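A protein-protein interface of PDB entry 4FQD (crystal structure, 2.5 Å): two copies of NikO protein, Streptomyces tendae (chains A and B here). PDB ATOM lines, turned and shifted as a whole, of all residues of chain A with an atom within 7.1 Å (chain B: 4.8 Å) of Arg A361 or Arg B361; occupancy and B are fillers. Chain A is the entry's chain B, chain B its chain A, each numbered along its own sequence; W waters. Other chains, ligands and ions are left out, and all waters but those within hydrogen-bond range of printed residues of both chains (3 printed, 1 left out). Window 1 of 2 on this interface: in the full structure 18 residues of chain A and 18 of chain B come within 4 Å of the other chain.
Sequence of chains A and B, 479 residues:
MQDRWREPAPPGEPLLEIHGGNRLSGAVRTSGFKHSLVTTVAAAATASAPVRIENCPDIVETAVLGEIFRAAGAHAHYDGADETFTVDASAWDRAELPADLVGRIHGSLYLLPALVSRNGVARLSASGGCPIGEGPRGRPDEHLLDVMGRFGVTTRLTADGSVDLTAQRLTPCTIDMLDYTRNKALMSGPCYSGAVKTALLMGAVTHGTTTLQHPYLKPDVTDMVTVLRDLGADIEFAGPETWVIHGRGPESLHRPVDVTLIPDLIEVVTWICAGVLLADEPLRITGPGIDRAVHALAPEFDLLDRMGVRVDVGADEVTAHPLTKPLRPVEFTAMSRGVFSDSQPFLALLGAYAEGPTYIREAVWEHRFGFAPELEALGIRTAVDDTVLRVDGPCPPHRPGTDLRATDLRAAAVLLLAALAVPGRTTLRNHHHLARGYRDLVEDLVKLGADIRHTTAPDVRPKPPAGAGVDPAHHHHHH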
ATOM      1  N   ARG A 182      35.268  -1.506 -13.918  1.00  0.00           N
ATOM      2  CA  ARG A 182      34.817  -2.102 -12.667  1.00  0.00           C
ATOM      3  C   ARG A 182      35.570  -3.400 -12.404  1.00  0.00           C
ATOM      4  O   ARG A 182      36.058  -3.634 -11.300  1.00  0.00           O
ATOM      5  CB  ARG A 182      33.310  -2.362 -12.691  1.00  0.00           C
ATOM      6  CG  ARG A 182      32.792  -3.026 -11.425  1.00  0.00           C
ATOM      7  CD  ARG A 182      31.314  -3.371 -11.518  1.00  0.00           C
ATOM      8  NE  ARG A 182      30.466  -2.184 -11.572  1.00  0.00           N
ATOM      9  CZ  ARG A 182      29.785  -1.800 -12.647  1.00  0.00           C
ATOM     10  NH1 ARG A 182      29.846  -2.513 -13.763  1.00  0.00           N
ATOM     11  NH2 ARG A 182      29.037  -0.706 -12.603  1.00  0.00           N
ATOM     12  N   ASN A 183      35.658  -4.241 -13.428  1.00  0.00           N
ATOM     13  CA  ASN A 183      36.420  -5.480 -13.341  1.00  0.00           C
ATOM     14  C   ASN A 183      37.575  -5.475 -14.338  1.00  0.00           C
ATOM     15  O   ASN A 183      37.362  -5.449 -15.550  1.00  0.00           O
ATOM     16  CB  ASN A 183      35.518  -6.690 -13.579  1.00  0.00           C
ATOM     17  CG  ASN A 183      36.197  -8.001 -13.228  1.00  0.00           C
ATOM     18  OD1 ASN A 183      36.987  -8.532 -14.008  1.00  0.00           O
ATOM     19  ND2 ASN A 183      35.890  -8.528 -12.049  1.00  0.00           N
ATOM     20  N   LEU A 186      37.865  -8.657 -16.668  1.00  0.00           N
ATOM     21  CA  LEU A 186      36.837  -8.641 -17.700  1.00  0.00           C
ATOM     22  C   LEU A 186      37.010  -7.429 -18.608  1.00  0.00           C
ATOM     23  O   LEU A 186      36.507  -7.410 -19.732  1.00  0.00           O
ATOM     24  CB  LEU A 186      35.445  -8.622 -17.068  1.00  0.00           C
ATOM     25  CG  LEU A 186      34.294  -9.067 -17.972  1.00  0.00           C
ATOM     26  CD1 LEU A 186      34.385 -10.561 -18.253  1.00  0.00           C
ATOM     27  CD2 LEU A 186      32.948  -8.711 -17.362  1.00  0.00           C
ATOM     28  N   GLU A 331      23.504 -18.202 -22.563  1.00  0.00           N
ATOM     29  CA  GLU A 331      24.030 -17.614 -21.343  1.00  0.00           C
ATOM     30  C   GLU A 331      25.190 -16.703 -21.722  1.00  0.00           C
ATOM     31  O   GLU A 331      26.174 -17.158 -22.306  1.00  0.00           O
ATOM     32  CB  GLU A 331      24.495 -18.718 -20.388  1.00  0.00           C
ATOM     33  CG  GLU A 331      25.169 -18.228 -19.118  1.00  0.00           C
ATOM     34  CD  GLU A 331      26.658 -17.994 -19.292  1.00  0.00           C
ATOM     35  OE1 GLU A 331      27.352 -18.906 -19.789  1.00  0.00           O
ATOM     36  OE2 GLU A 331      27.131 -16.894 -18.940  1.00  0.00           O
ATOM     37  N   PHE A 332      25.076 -15.420 -21.401  1.00  0.00           N
ATOM     38  CA  PHE A 332      26.123 -14.470 -21.761  1.00  0.00           C
ATOM     39  C   PHE A 332      26.208 -13.294 -20.796  1.00  0.00           C
ATOM     40  O   PHE A 332      25.355 -13.124 -19.924  1.00  0.00           O
ATOM     41  CB  PHE A 332      25.929 -13.961 -23.193  1.00  0.00           C
ATOM     42  CG  PHE A 332      24.758 -13.029 -23.357  1.00  0.00           C
ATOM     43  CD1 PHE A 332      23.475 -13.528 -23.513  1.00  0.00           C
ATOM     44  CD2 PHE A 332      24.945 -11.654 -23.368  1.00  0.00           C
ATOM     45  CE1 PHE A 332      22.398 -12.673 -23.667  1.00  0.00           C
ATOM     46  CE2 PHE A 332      23.872 -10.795 -23.522  1.00  0.00           C
ATOM     47  CZ  PHE A 332      22.597 -11.305 -23.671  1.00  0.00           C
ATOM     48  N   THR A 333      27.245 -12.483 -20.971  1.00  0.00           N
ATOM     49  CA  THR A 333      27.444 -11.298 -20.153  1.00  0.00           C
ATOM     50  C   THR A 333      27.638 -10.073 -21.039  1.00  0.00           C
ATOM     51  O   THR A 333      28.523 -10.051 -21.896  1.00  0.00           O
ATOM     52  CB  THR A 333      28.673 -11.449 -19.232  1.00  0.00           C
ATOM     53  OG1 THR A 333      28.492 -12.577 -18.367  1.00  0.00           O
ATOM     54  CG2 THR A 333      28.866 -10.198 -18.392  1.00  0.00           C
ATOM     55  N   ALA A 334      26.802  -9.059 -20.839  1.00  0.00           N
ATOM     56  CA  ALA A 334      26.954  -7.802 -21.558  1.00  0.00           C
ATOM     57  C   ALA A 334      28.124  -7.027 -20.969  1.00  0.00           C
ATOM     58  O   ALA A 334      28.066  -6.577 -19.825  1.00  0.00           O
ATOM     59  CB  ALA A 334      25.678  -6.985 -21.482  1.00  0.00           C
ATOM     60  N   MET A 335      29.187  -6.880 -21.752  1.00  0.00           N
ATOM     61  CA  MET A 335      30.408  -6.251 -21.269  1.00  0.00           C
ATOM     62  C   MET A 335      31.019  -5.306 -22.299  1.00  0.00           C
ATOM     63  O   MET A 335      30.609  -5.284 -23.461  1.00  0.00           O
ATOM     64  CB  MET A 335      31.425  -7.318 -20.863  1.00  0.00           C
ATOM     65  CG  MET A 335      31.732  -8.316 -21.963  1.00  0.00           C
ATOM     66  SD  MET A 335      32.757  -9.684 -21.397  1.00  0.00           S
ATOM     67  CE  MET A 335      33.049 -10.538 -22.945  1.00  0.00           C
ATOM     68  N   VAL A 339      29.347  -8.089 -25.725  1.00  0.00           N
ATOM     69  CA  VAL A 339      28.003  -7.683 -26.115  1.00  0.00           C
ATOM     70  C   VAL A 339      27.650  -6.320 -25.530  1.00  0.00           C
ATOM     71  O   VAL A 339      27.837  -6.084 -24.336  1.00  0.00           O
ATOM     72  CB  VAL A 339      26.955  -8.716 -25.654  1.00  0.00           C
ATOM     73  CG1 VAL A 339      25.553  -8.260 -26.027  1.00  0.00           C
ATOM     74  CG2 VAL A 339      27.259 -10.081 -26.256  1.00  0.00           C
ATOM     75  N   GLN A 344      21.333  -6.135 -25.105  1.00  0.00           N
ATOM     76  CA  GLN A 344      20.685  -7.165 -24.280  1.00  0.00           C
ATOM     77  C   GLN A 344      19.149  -7.128 -24.118  1.00  0.00           C
ATOM     78  O   GLN A 344      18.535  -8.189 -23.993  1.00  0.00           O
ATOM     79  CB  GLN A 344      21.385  -7.317 -22.916  1.00  0.00           C
ATOM     80  CG  GLN A 344      21.643  -6.030 -22.153  1.00  0.00           C
ATOM     81  CD  GLN A 344      20.565  -5.717 -21.132  1.00  0.00           C
ATOM     82  OE1 GLN A 344      19.472  -6.279 -21.175  1.00  0.00           O
ATOM     83  NE2 GLN A 344      20.873  -4.819 -20.204  1.00  0.00           N
ATOM     84  N   TYR A 359      20.079 -16.631 -19.624  1.00  0.00           N
ATOM     85  CA  TYR A 359      20.715 -15.881 -18.548  1.00  0.00           C
ATOM     86  C   TYR A 359      21.473 -14.675 -19.087  1.00  0.00           C
ATOM     87  O   TYR A 359      22.361 -14.812 -19.930  1.00  0.00           O
ATOM     88  CB  TYR A 359      21.662 -16.782 -17.756  1.00  0.00           C
ATOM     89  CG  TYR A 359      20.998 -18.014 -17.182  1.00  0.00           C
ATOM     90  CD1 TYR A 359      20.950 -19.200 -17.902  1.00  0.00           C
ATOM     91  CD2 TYR A 359      20.420 -17.989 -15.920  1.00  0.00           C
ATOM     92  CE1 TYR A 359      20.346 -20.327 -17.382  1.00  0.00           C
ATOM     93  CE2 TYR A 359      19.813 -19.111 -15.391  1.00  0.00           C
ATOM     94  CZ  TYR A 359      19.779 -20.277 -16.125  1.00  0.00           C
ATOM     95  OH  TYR A 359      19.178 -21.396 -15.601  1.00  0.00           O
ATOM     96  N   ILE A 360      21.119 -13.494 -18.593  1.00  0.00           N
ATOM     97  CA  ILE A 360      21.749 -12.260 -19.038  1.00  0.00           C
ATOM     98  C   ILE A 360      22.373 -11.508 -17.868  1.00  0.00           C
ATOM     99  O   ILE A 360      21.670 -11.049 -16.969  1.00  0.00           O
ATOM    100  CB  ILE A 360      20.738 -11.335 -19.744  1.00  0.00           C
ATOM    101  CG1 ILE A 360      20.051 -12.072 -20.894  1.00  0.00           C
ATOM    102  CG2 ILE A 360      21.429 -10.073 -20.242  1.00  0.00           C
ATOM    103  CD1 ILE A 360      19.017 -11.241 -21.621  1.00  0.00           C
ATOM    104  N   ARG A 361      23.697 -11.388 -17.883  1.00  0.00           N
ATOM    105  CA  ARG A 361      24.398 -10.633 -16.854  1.00  0.00           C
ATOM    106  C   ARG A 361      24.895  -9.297 -17.397  1.00  0.00           C
ATOM    107  O   ARG A 361      25.505  -9.236 -18.465  1.00  0.00           O
ATOM    108  CB  ARG A 361      25.570 -11.434 -16.283  1.00  0.00           C
ATOM    109  CG  ARG A 361      26.295 -10.723 -15.150  1.00  0.00           C
ATOM    110  CD  ARG A 361      27.538 -11.478 -14.715  1.00  0.00           C
ATOM    111  NE  ARG A 361      27.223 -12.765 -14.103  1.00  0.00           N
ATOM    112  CZ  ARG A 361      27.083 -12.956 -12.795  1.00  0.00           C
ATOM    113  NH1 ARG A 361      27.227 -11.943 -11.953  1.00  0.00           N
ATOM    114  NH2 ARG A 361      26.798 -14.163 -12.327  1.00  0.00           N
ATOM    115  N   GLU A 362      24.626  -8.231 -16.653  1.00  0.00           N
ATOM    116  CA  GLU A 362      25.055  -6.895 -17.042  1.00  0.00           C
ATOM    117  C   GLU A 362      26.347  -6.513 -16.327  1.00  0.00           C
ATOM    118  O   GLU A 362      26.398  -6.480 -15.097  1.00  0.00           O
ATOM    119  CB  GLU A 362      23.958  -5.878 -16.728  1.00  0.00           C
ATOM    120  CG  GLU A 362      24.346  -4.445 -17.017  1.00  0.00           C
ATOM    121  CD  GLU A 362      24.553  -4.179 -18.492  1.00  0.00           C
ATOM    122  OE1 GLU A 362      23.570  -4.266 -19.259  1.00  0.00           O
ATOM    123  OE2 GLU A 362      25.698  -3.881 -18.885  1.00  0.00           O
ATOM    124  N   ALA A 363      27.391  -6.228 -17.099  1.00  0.00           N
ATOM    125  CA  ALA A 363      28.687  -5.879 -16.526  1.00  0.00           C
ATOM    126  C   ALA A 363      29.130  -4.471 -16.912  1.00  0.00           C
ATOM    127  O   ALA A 363      30.318  -4.152 -16.864  1.00  0.00           O
ATOM    128  CB  ALA A 363      29.740  -6.897 -16.933  1.00  0.00           C
ATOM    129  N   VAL A 364      28.173  -3.635 -17.303  1.00  0.00           N
ATOM    130  CA  VAL A 364      28.461  -2.242 -17.625  1.00  0.00           C
ATOM    131  C   VAL A 364      27.576  -1.307 -16.802  1.00  0.00           C
ATOM    132  O   VAL A 364      28.069  -0.547 -15.970  1.00  0.00           O
ATOM    133  CB  VAL A 364      28.259  -1.941 -19.125  1.00  0.00           C
ATOM    134  CG1 VAL A 364      28.655  -0.504 -19.432  1.00  0.00           C
ATOM    135  CG2 VAL A 364      29.059  -2.911 -19.979  1.00  0.00           C
ATOM    136  N   GLU A 366      25.031  -1.753 -14.202  1.00  0.00           N
ATOM    137  CA  GLU A 366      24.471  -2.706 -13.231  1.00  0.00           C
ATOM    138  C   GLU A 366      22.949  -2.860 -13.207  1.00  0.00           C
ATOM    139  O   GLU A 366      22.428  -3.939 -13.479  1.00  0.00           O
ATOM    140  CB  GLU A 366      24.978  -2.379 -11.824  1.00  0.00           C
ATOM    141  CG  GLU A 366      26.469  -2.591 -11.641  1.00  0.00           C
ATOM    142  CD  GLU A 366      26.785  -3.748 -10.715  1.00  0.00           C
ATOM    143  OE1 GLU A 366      27.764  -4.477 -10.983  1.00  0.00           O
ATOM    144  OE2 GLU A 366      26.055  -3.926  -9.717  1.00  0.00           O
ATOM    145  N   PHE A 369      17.587  -3.217 -16.054  1.00  0.00           N
ATOM    146  CA  PHE A 369      16.550  -4.158 -16.452  1.00  0.00           C
ATOM    147  C   PHE A 369      15.175  -3.567 -16.169  1.00  0.00           C
ATOM    148  O   PHE A 369      14.264  -4.266 -15.729  1.00  0.00           O
ATOM    149  CB  PHE A 369      16.718  -5.494 -15.724  1.00  0.00           C
ATOM    150  CG  PHE A 369      18.032  -6.170 -15.997  1.00  0.00           C
ATOM    151  CD1 PHE A 369      18.384  -6.532 -17.286  1.00  0.00           C
ATOM    152  CD2 PHE A 369      18.911  -6.452 -14.964  1.00  0.00           C
ATOM    153  CE1 PHE A 369      19.593  -7.154 -17.544  1.00  0.00           C
ATOM    154  CE2 PHE A 369      20.120  -7.076 -15.214  1.00  0.00           C
ATOM    155  CZ  PHE A 369      20.459  -7.428 -16.507  1.00  0.00           C
ATOM    156  N   ASP A 385      17.825 -10.560 -10.300  1.00  0.00           N
ATOM    157  CA  ASP A 385      18.581 -10.505  -9.057  1.00  0.00           C
ATOM    158  C   ASP A 385      19.875  -9.734  -9.287  1.00  0.00           C
ATOM    159  O   ASP A 385      20.812 -10.250  -9.899  1.00  0.00           O
ATOM    160  CB  ASP A 385      18.886 -11.913  -8.541  1.00  0.00           C
ATOM    161  CG  ASP A 385      19.395 -11.915  -7.108  1.00  0.00           C
ATOM    162  OD1 ASP A 385      19.673 -10.825  -6.562  1.00  0.00           O
ATOM    163  OD2 ASP A 385      19.523 -13.012  -6.525  1.00  0.00           O
ATOM    164  N   ASP A 386      19.908  -8.497  -8.797  1.00  0.00           N
ATOM    165  CA  ASP A 386      21.071  -7.620  -8.922  1.00  0.00           C
ATOM    166  C   ASP A 386      21.461  -7.364 -10.380  1.00  0.00           C
ATOM    167  O   ASP A 386      20.796  -6.604 -11.083  1.00  0.00           O
ATOM    168  CB  ASP A 386      22.261  -8.172  -8.127  1.00  0.00           C
ATOM    169  CG  ASP A 386      23.385  -7.164  -7.983  1.00  0.00           C
ATOM    170  OD1 ASP A 386      23.106  -5.947  -8.038  1.00  0.00           O
ATOM    171  OD2 ASP A 386      24.548  -7.589  -7.811  1.00  0.00           O
ATOM    172  N   THR A 387      22.534  -8.009 -10.826  1.00  0.00           N
ATOM    173  CA  THR A 387      23.071  -7.775 -12.162  1.00  0.00           C
ATOM    174  C   THR A 387      22.649  -8.855 -13.151  1.00  0.00           C
ATOM    175  O   THR A 387      23.053  -8.832 -14.315  1.00  0.00           O
ATOM    176  CB  THR A 387      24.609  -7.716 -12.136  1.00  0.00           C
ATOM    177  OG1 THR A 387      25.132  -8.996 -11.762  1.00  0.00           O
ATOM    178  CG2 THR A 387      25.080  -6.677 -11.142  1.00  0.00           C
ATOM    179  N   VAL A 388      21.838  -9.799 -12.687  1.00  0.00           N
ATOM    180  CA  VAL A 388      21.454 -10.940 -13.509  1.00  0.00           C
ATOM    181  C   VAL A 388      19.970 -10.945 -13.868  1.00  0.00           C
ATOM    182  O   VAL A 388      19.106 -10.830 -12.998  1.00  0.00           O
ATOM    183  CB  VAL A 388      21.820 -12.271 -12.819  1.00  0.00           C
ATOM    184  CG1 VAL A 388      21.226 -13.451 -13.575  1.00  0.00           C
ATOM    185  CG2 VAL A 388      23.333 -12.408 -12.702  1.00  0.00           C
ATOM    186  N   LEU A 389      19.689 -11.075 -15.160  1.00  0.00           N
ATOM    187  CA  LEU A 389      18.326 -11.238 -15.648  1.00  0.00           C
ATOM    188  C   LEU A 389      18.159 -12.618 -16.273  1.00  0.00           C
ATOM    189  O   LEU A 389      18.998 -13.059 -17.060  1.00  0.00           O
ATOM    190  CB  LEU A 389      17.990 -10.157 -16.678  1.00  0.00           C
ATOM    191  CG  LEU A 389      16.746 -10.394 -17.538  1.00  0.00           C
ATOM    192  CD1 LEU A 389      15.488 -10.365 -16.688  1.00  0.00           C
ATOM    193  CD2 LEU A 389      16.661  -9.379 -18.668  1.00  0.00           C
ATOM    194  N   LEU B 186      19.998 -16.390 -11.341  1.00  0.00           N
ATOM    195  CA  LEU B 186      20.947 -17.288 -11.981  1.00  0.00           C
ATOM    196  C   LEU B 186      20.793 -18.701 -11.427  1.00  0.00           C
ATOM    197  O   LEU B 186      21.227 -19.673 -12.050  1.00  0.00           O
ATOM    198  CB  LEU B 186      22.377 -16.791 -11.763  1.00  0.00           C
ATOM    199  CG  LEU B 186      23.445 -17.323 -12.719  1.00  0.00           C
ATOM    200  CD1 LEU B 186      23.230 -16.764 -14.118  1.00  0.00           C
ATOM    201  CD2 LEU B 186      24.841 -16.991 -12.213  1.00  0.00           C
ATOM    202  N   PHE B 332      31.898 -17.213 -20.707  1.00  0.00           N
ATOM    203  CA  PHE B 332      30.842 -17.966 -20.045  1.00  0.00           C
ATOM    204  C   PHE B 332      30.914 -17.824 -18.533  1.00  0.00           C
ATOM    205  O   PHE B 332      31.854 -17.241 -17.992  1.00  0.00           O
ATOM    206  CB  PHE B 332      30.915 -19.446 -20.430  1.00  0.00           C
ATOM    207  CG  PHE B 332      32.147 -20.144 -19.928  1.00  0.00           C
ATOM    208  CD1 PHE B 332      33.324 -20.110 -20.657  1.00  0.00           C
ATOM    209  CD2 PHE B 332      32.127 -20.837 -18.729  1.00  0.00           C
ATOM    210  CE1 PHE B 332      34.459 -20.750 -20.198  1.00  0.00           C
ATOM    211  CE2 PHE B 332      33.258 -21.478 -18.264  1.00  0.00           C
ATOM    212  CZ  PHE B 332      34.427 -21.435 -19.001  1.00  0.00           C
ATOM    213  N   THR B 333      29.914 -18.374 -17.857  1.00  0.00           N
ATOM    214  CA  THR B 333      29.855 -18.323 -16.406  1.00  0.00           C
ATOM    215  C   THR B 333      29.640 -19.714 -15.826  1.00  0.00           C
ATOM    216  O   THR B 333      28.650 -20.376 -16.132  1.00  0.00           O
ATOM    217  CB  THR B 333      28.721 -17.399 -15.925  1.00  0.00           C
ATOM    218  OG1 THR B 333      28.955 -16.066 -16.397  1.00  0.00           O
ATOM    219  CG2 THR B 333      28.651 -17.389 -14.410  1.00  0.00           C
ATOM    220  N   ALA B 334      30.576 -20.158 -14.996  1.00  0.00           N
ATOM    221  CA  ALA B 334      30.422 -21.423 -14.292  1.00  0.00           C
ATOM    222  C   ALA B 334      29.346 -21.273 -13.222  1.00  0.00           C
ATOM    223  O   ALA B 334      29.509 -20.509 -12.272  1.00  0.00           O
ATOM    224  CB  ALA B 334      31.740 -21.851 -13.670  1.00  0.00           C
ATOM    225  N   TYR B 359      36.919 -15.356 -21.494  1.00  0.00           N
ATOM    226  CA  TYR B 359      36.445 -14.792 -20.238  1.00  0.00           C
ATOM    227  C   TYR B 359      35.711 -15.839 -19.412  1.00  0.00           C
ATOM    228  O   TYR B 359      34.716 -16.410 -19.857  1.00  0.00           O
ATOM    229  CB  TYR B 359      35.534 -13.591 -20.499  1.00  0.00           C
ATOM    230  CG  TYR B 359      36.180 -12.502 -21.325  1.00  0.00           C
ATOM    231  CD1 TYR B 359      36.112 -12.524 -22.712  1.00  0.00           C
ATOM    232  CD2 TYR B 359      36.856 -11.452 -20.718  1.00  0.00           C
ATOM    233  CE1 TYR B 359      36.700 -11.532 -23.472  1.00  0.00           C
ATOM    234  CE2 TYR B 359      37.448 -10.453 -21.469  1.00  0.00           C
ATOM    235  CZ  TYR B 359      37.366 -10.499 -22.846  1.00  0.00           C
ATOM    236  OH  TYR B 359      37.953  -9.508 -23.599  1.00  0.00           O
ATOM    237  N   ILE B 360      36.208 -16.089 -18.207  1.00  0.00           N
ATOM    238  CA  ILE B 360      35.615 -17.089 -17.329  1.00  0.00           C
ATOM    239  C   ILE B 360      35.129 -16.465 -16.027  1.00  0.00           C
ATOM    240  O   ILE B 360      35.910 -15.864 -15.287  1.00  0.00           O
ATOM    241  CB  ILE B 360      36.616 -18.215 -17.007  1.00  0.00           C
ATOM    242  CG1 ILE B 360      37.079 -18.899 -18.296  1.00  0.00           C
ATOM    243  CG2 ILE B 360      35.994 -19.220 -16.048  1.00  0.00           C
ATOM    244  CD1 ILE B 360      38.097 -19.996 -18.078  1.00  0.00           C
ATOM    245  N   ARG B 361      33.837 -16.605 -15.753  1.00  0.00           N
ATOM    246  CA  ARG B 361      33.262 -16.071 -14.525  1.00  0.00           C
ATOM    247  C   ARG B 361      32.817 -17.184 -13.586  1.00  0.00           C
ATOM    248  O   ARG B 361      32.098 -18.100 -13.986  1.00  0.00           O
ATOM    249  CB  ARG B 361      32.080 -15.152 -14.835  1.00  0.00           C
ATOM    250  CG  ARG B 361      31.632 -14.320 -13.647  1.00  0.00           C
ATOM    251  CD  ARG B 361      30.430 -13.470 -13.998  1.00  0.00           C
ATOM    252  NE  ARG B 361      30.405 -12.227 -13.235  1.00  0.00           N
ATOM    253  CZ  ARG B 361      30.873 -11.068 -13.683  1.00  0.00           C
ATOM    254  NH1 ARG B 361      31.396 -10.989 -14.897  1.00  0.00           N
ATOM    255  NH2 ARG B 361      30.812  -9.985 -12.921  1.00  0.00           N
ATOM    256  N   GLU B 362      33.248 -17.092 -12.333  1.00  0.00           N
ATOM    257  CA  GLU B 362      32.893 -18.073 -11.318  1.00  0.00           C
ATOM    258  C   GLU B 362      31.673 -17.617 -10.525  1.00  0.00           C
ATOM    259  O   GLU B 362      31.690 -16.554  -9.904  1.00  0.00           O
ATOM    260  CB  GLU B 362      34.074 -18.300 -10.375  1.00  0.00           C
ATOM    261  CG  GLU B 362      33.751 -19.175  -9.184  1.00  0.00           C
ATOM    262  CD  GLU B 362      33.447 -20.604  -9.576  1.00  0.00           C
ATOM    263  OE1 GLU B 362      34.301 -21.236 -10.231  1.00  0.00           O
ATOM    264  OE2 GLU B 362      32.350 -21.093  -9.233  1.00  0.00           O
ATOM    265  N   ALA B 363      30.616 -18.423 -10.543  1.00  0.00           N
ATOM    266  CA  ALA B 363      29.382 -18.070  -9.848  1.00  0.00           C
ATOM    267  C   ALA B 363      28.946 -19.141  -8.851  1.00  0.00           C
ATOM    268  O   ALA B 363      27.777 -19.206  -8.473  1.00  0.00           O
ATOM    269  CB  ALA B 363      28.271 -17.791 -10.847  1.00  0.00           C
ATOM    270  N   THR B 387      35.757 -12.471  -9.249  1.00  0.00           N
ATOM    271  CA  THR B 387      35.071 -13.661  -9.745  1.00  0.00           C
ATOM    272  C   THR B 387      35.410 -13.953 -11.198  1.00  0.00           C
ATOM    273  O   THR B 387      34.913 -14.923 -11.771  1.00  0.00           O
ATOM    274  CB  THR B 387      33.541 -13.501  -9.675  1.00  0.00           C
ATOM    275  OG1 THR B 387      33.105 -12.646 -10.739  1.00  0.00           O
ATOM    276  CG2 THR B 387      33.117 -12.896  -8.354  1.00  0.00           C
ATOM    277  N   VAL B 388      36.244 -13.113 -11.800  1.00  0.00           N
ATOM    278  CA  VAL B 388      36.507 -13.210 -13.231  1.00  0.00           C
ATOM    279  C   VAL B 388      37.945 -13.604 -13.548  1.00  0.00           C
ATOM    280  O   VAL B 388      38.892 -13.049 -12.993  1.00  0.00           O
ATOM    281  CB  VAL B 388      36.169 -11.884 -13.948  1.00  0.00           C
ATOM    282  CG1 VAL B 388      36.564 -11.945 -15.420  1.00  0.00           C
ATOM    283  CG2 VAL B 388      34.691 -11.570 -13.799  1.00  0.00           C
HETATM  284  O   HOH W   1      26.699 -14.776 -15.452  1.00  0.00           O
HETATM  285  O   HOH W   2      28.053  -9.103 -11.888  1.00  0.00           O
HETATM  286  O   HOH W   3      30.980 -12.576 -17.078  1.00  0.00           O
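The guanidinium group of Arg B361 sits close to the guanidinium group of Arg A361 (3.3 Å). OG1 of Thr B333 sits at hydrogen-bond distance from OE2 of Glu A331, at 3.2 Å.
The backbone NH of Phe B332 sits at hydrogen-bond distance from the backbone carbonyl oxygen of Tyr B359 (3.1 Å). The backbone NH (N) of Leu A186 lies within hydrogen-bond range of the side-chain amide oxygen (OD1) of Asn A183 (2.8 Å). The backbone NH (N) of Arg A361 sits at hydrogen-bond distance from the backbone carbonyl oxygen (O) of Phe A332 (3.2 Å). O of Arg B361 sits at hydrogen-bond distance from N of Ala B334, at 2.8 Å. The backbone NH (N) of Ala A334 lies within hydrogen-bond range of the backbone carbonyl oxygen (O) of Arg A361. O of Phe B332 is in hydrogen-bond range of N of Arg B361, 3.1 Å away.
Among the printed residues, merely in contact across the chains: Arg A361 with Leu B186 (3.4 Å), Asn A183 with Val B388 (3.5 Å), Tyr A359 with Leu B186 (3.6 Å), Leu A186 with Tyr B359 (3.6 Å), Glu A331 with Phe B332 (3.6 Å), Met A335 with Tyr B359 (3.7 Å), Leu A186 with Arg B361 (3.7 Å), Leu A186 with Val B388 (3.7 Å) and Val A388 with Leu B186 (3.9 Å).
Arg B361 touches just these residues of chain A: Leu A186 and Arg A361. Printed residues of chain A within 4 Å of Leu B186: Tyr A359, Arg A361 and Val A388. Printed residues of chain A within 4 Å of Val B388: Asn A183 (3.5 Å) and Leu A186 (3.7 Å). Printed residues of chain A within 4 Å of Tyr B359: Leu A186 and Met A335. Of the printed residues of chain B, Tyr A359 touches Leu B186. Phe A369 touches none of the printed residues of chain B. The nearest residue of chain B that does not touch Arg A361 is Ala B363 (4.2 Å). The nearest residue of chain A that does not touch Arg B361 is Thr A333 (4.4 Å).
Of the 11 printed residues of chain B, 6 touch a printed residue of chain A. Hydrophobic or aromatic side chains of chain B that line the printed part of chain A: Leu B186, Phe B332, Tyr B359 and Val B388. Along chain B the printed residues that touch a printed residue of chain A span positions 186 to 388. Printed residues of chain A that touch a printed residue of chain B: Asn A183, Leu A186, Glu A331, Met A335, Tyr A359, Arg A361 and Val A388. Hydrophobic or aromatic side chains of chain A within 4 Å of the printed part of chain B: Leu A186, Met A335, Tyr A359 and Val A388. Among the printed residues, no Asp or Glu carboxylate lies within 4 Å of a Lys or Arg side-chain nitrogen of the other chain.
Leu A186 touches Tyr B359, and with the chains exchanged Tyr A359 touches Leu B186. Leu A186 touches Arg B361, and with the chains exchanged Arg A361 touches Leu B186. Leu A186 touches Val B388, and with the chains exchanged Val A388 touches Leu B186. Arg B361 touches its own counterpart, Arg A361. Of the 11 pairs that touch across the chains among the printed residues, 7 have their exchanged pair printed and touching as well.
Water W1 lies within hydrogen-bond range of the guanidinium group (NE) of Arg A361 (2.5 Å) and the side-chain hydroxyl (OG1) of Thr B333 (2.8 Å). Water W3 lies within hydrogen-bond range of NH1 of Arg B361 (2.7 Å) and OG1 of Thr A333 (2.8 Å). Water W2 lies within hydrogen-bond range of the side-chain hydroxyl (OG1) of Thr A387 (2.9 Å), the guanidinium group (NH1) of Arg A361 (3.0 Å) and the guanidinium group (NH2) of Arg B361 (3.1 Å).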
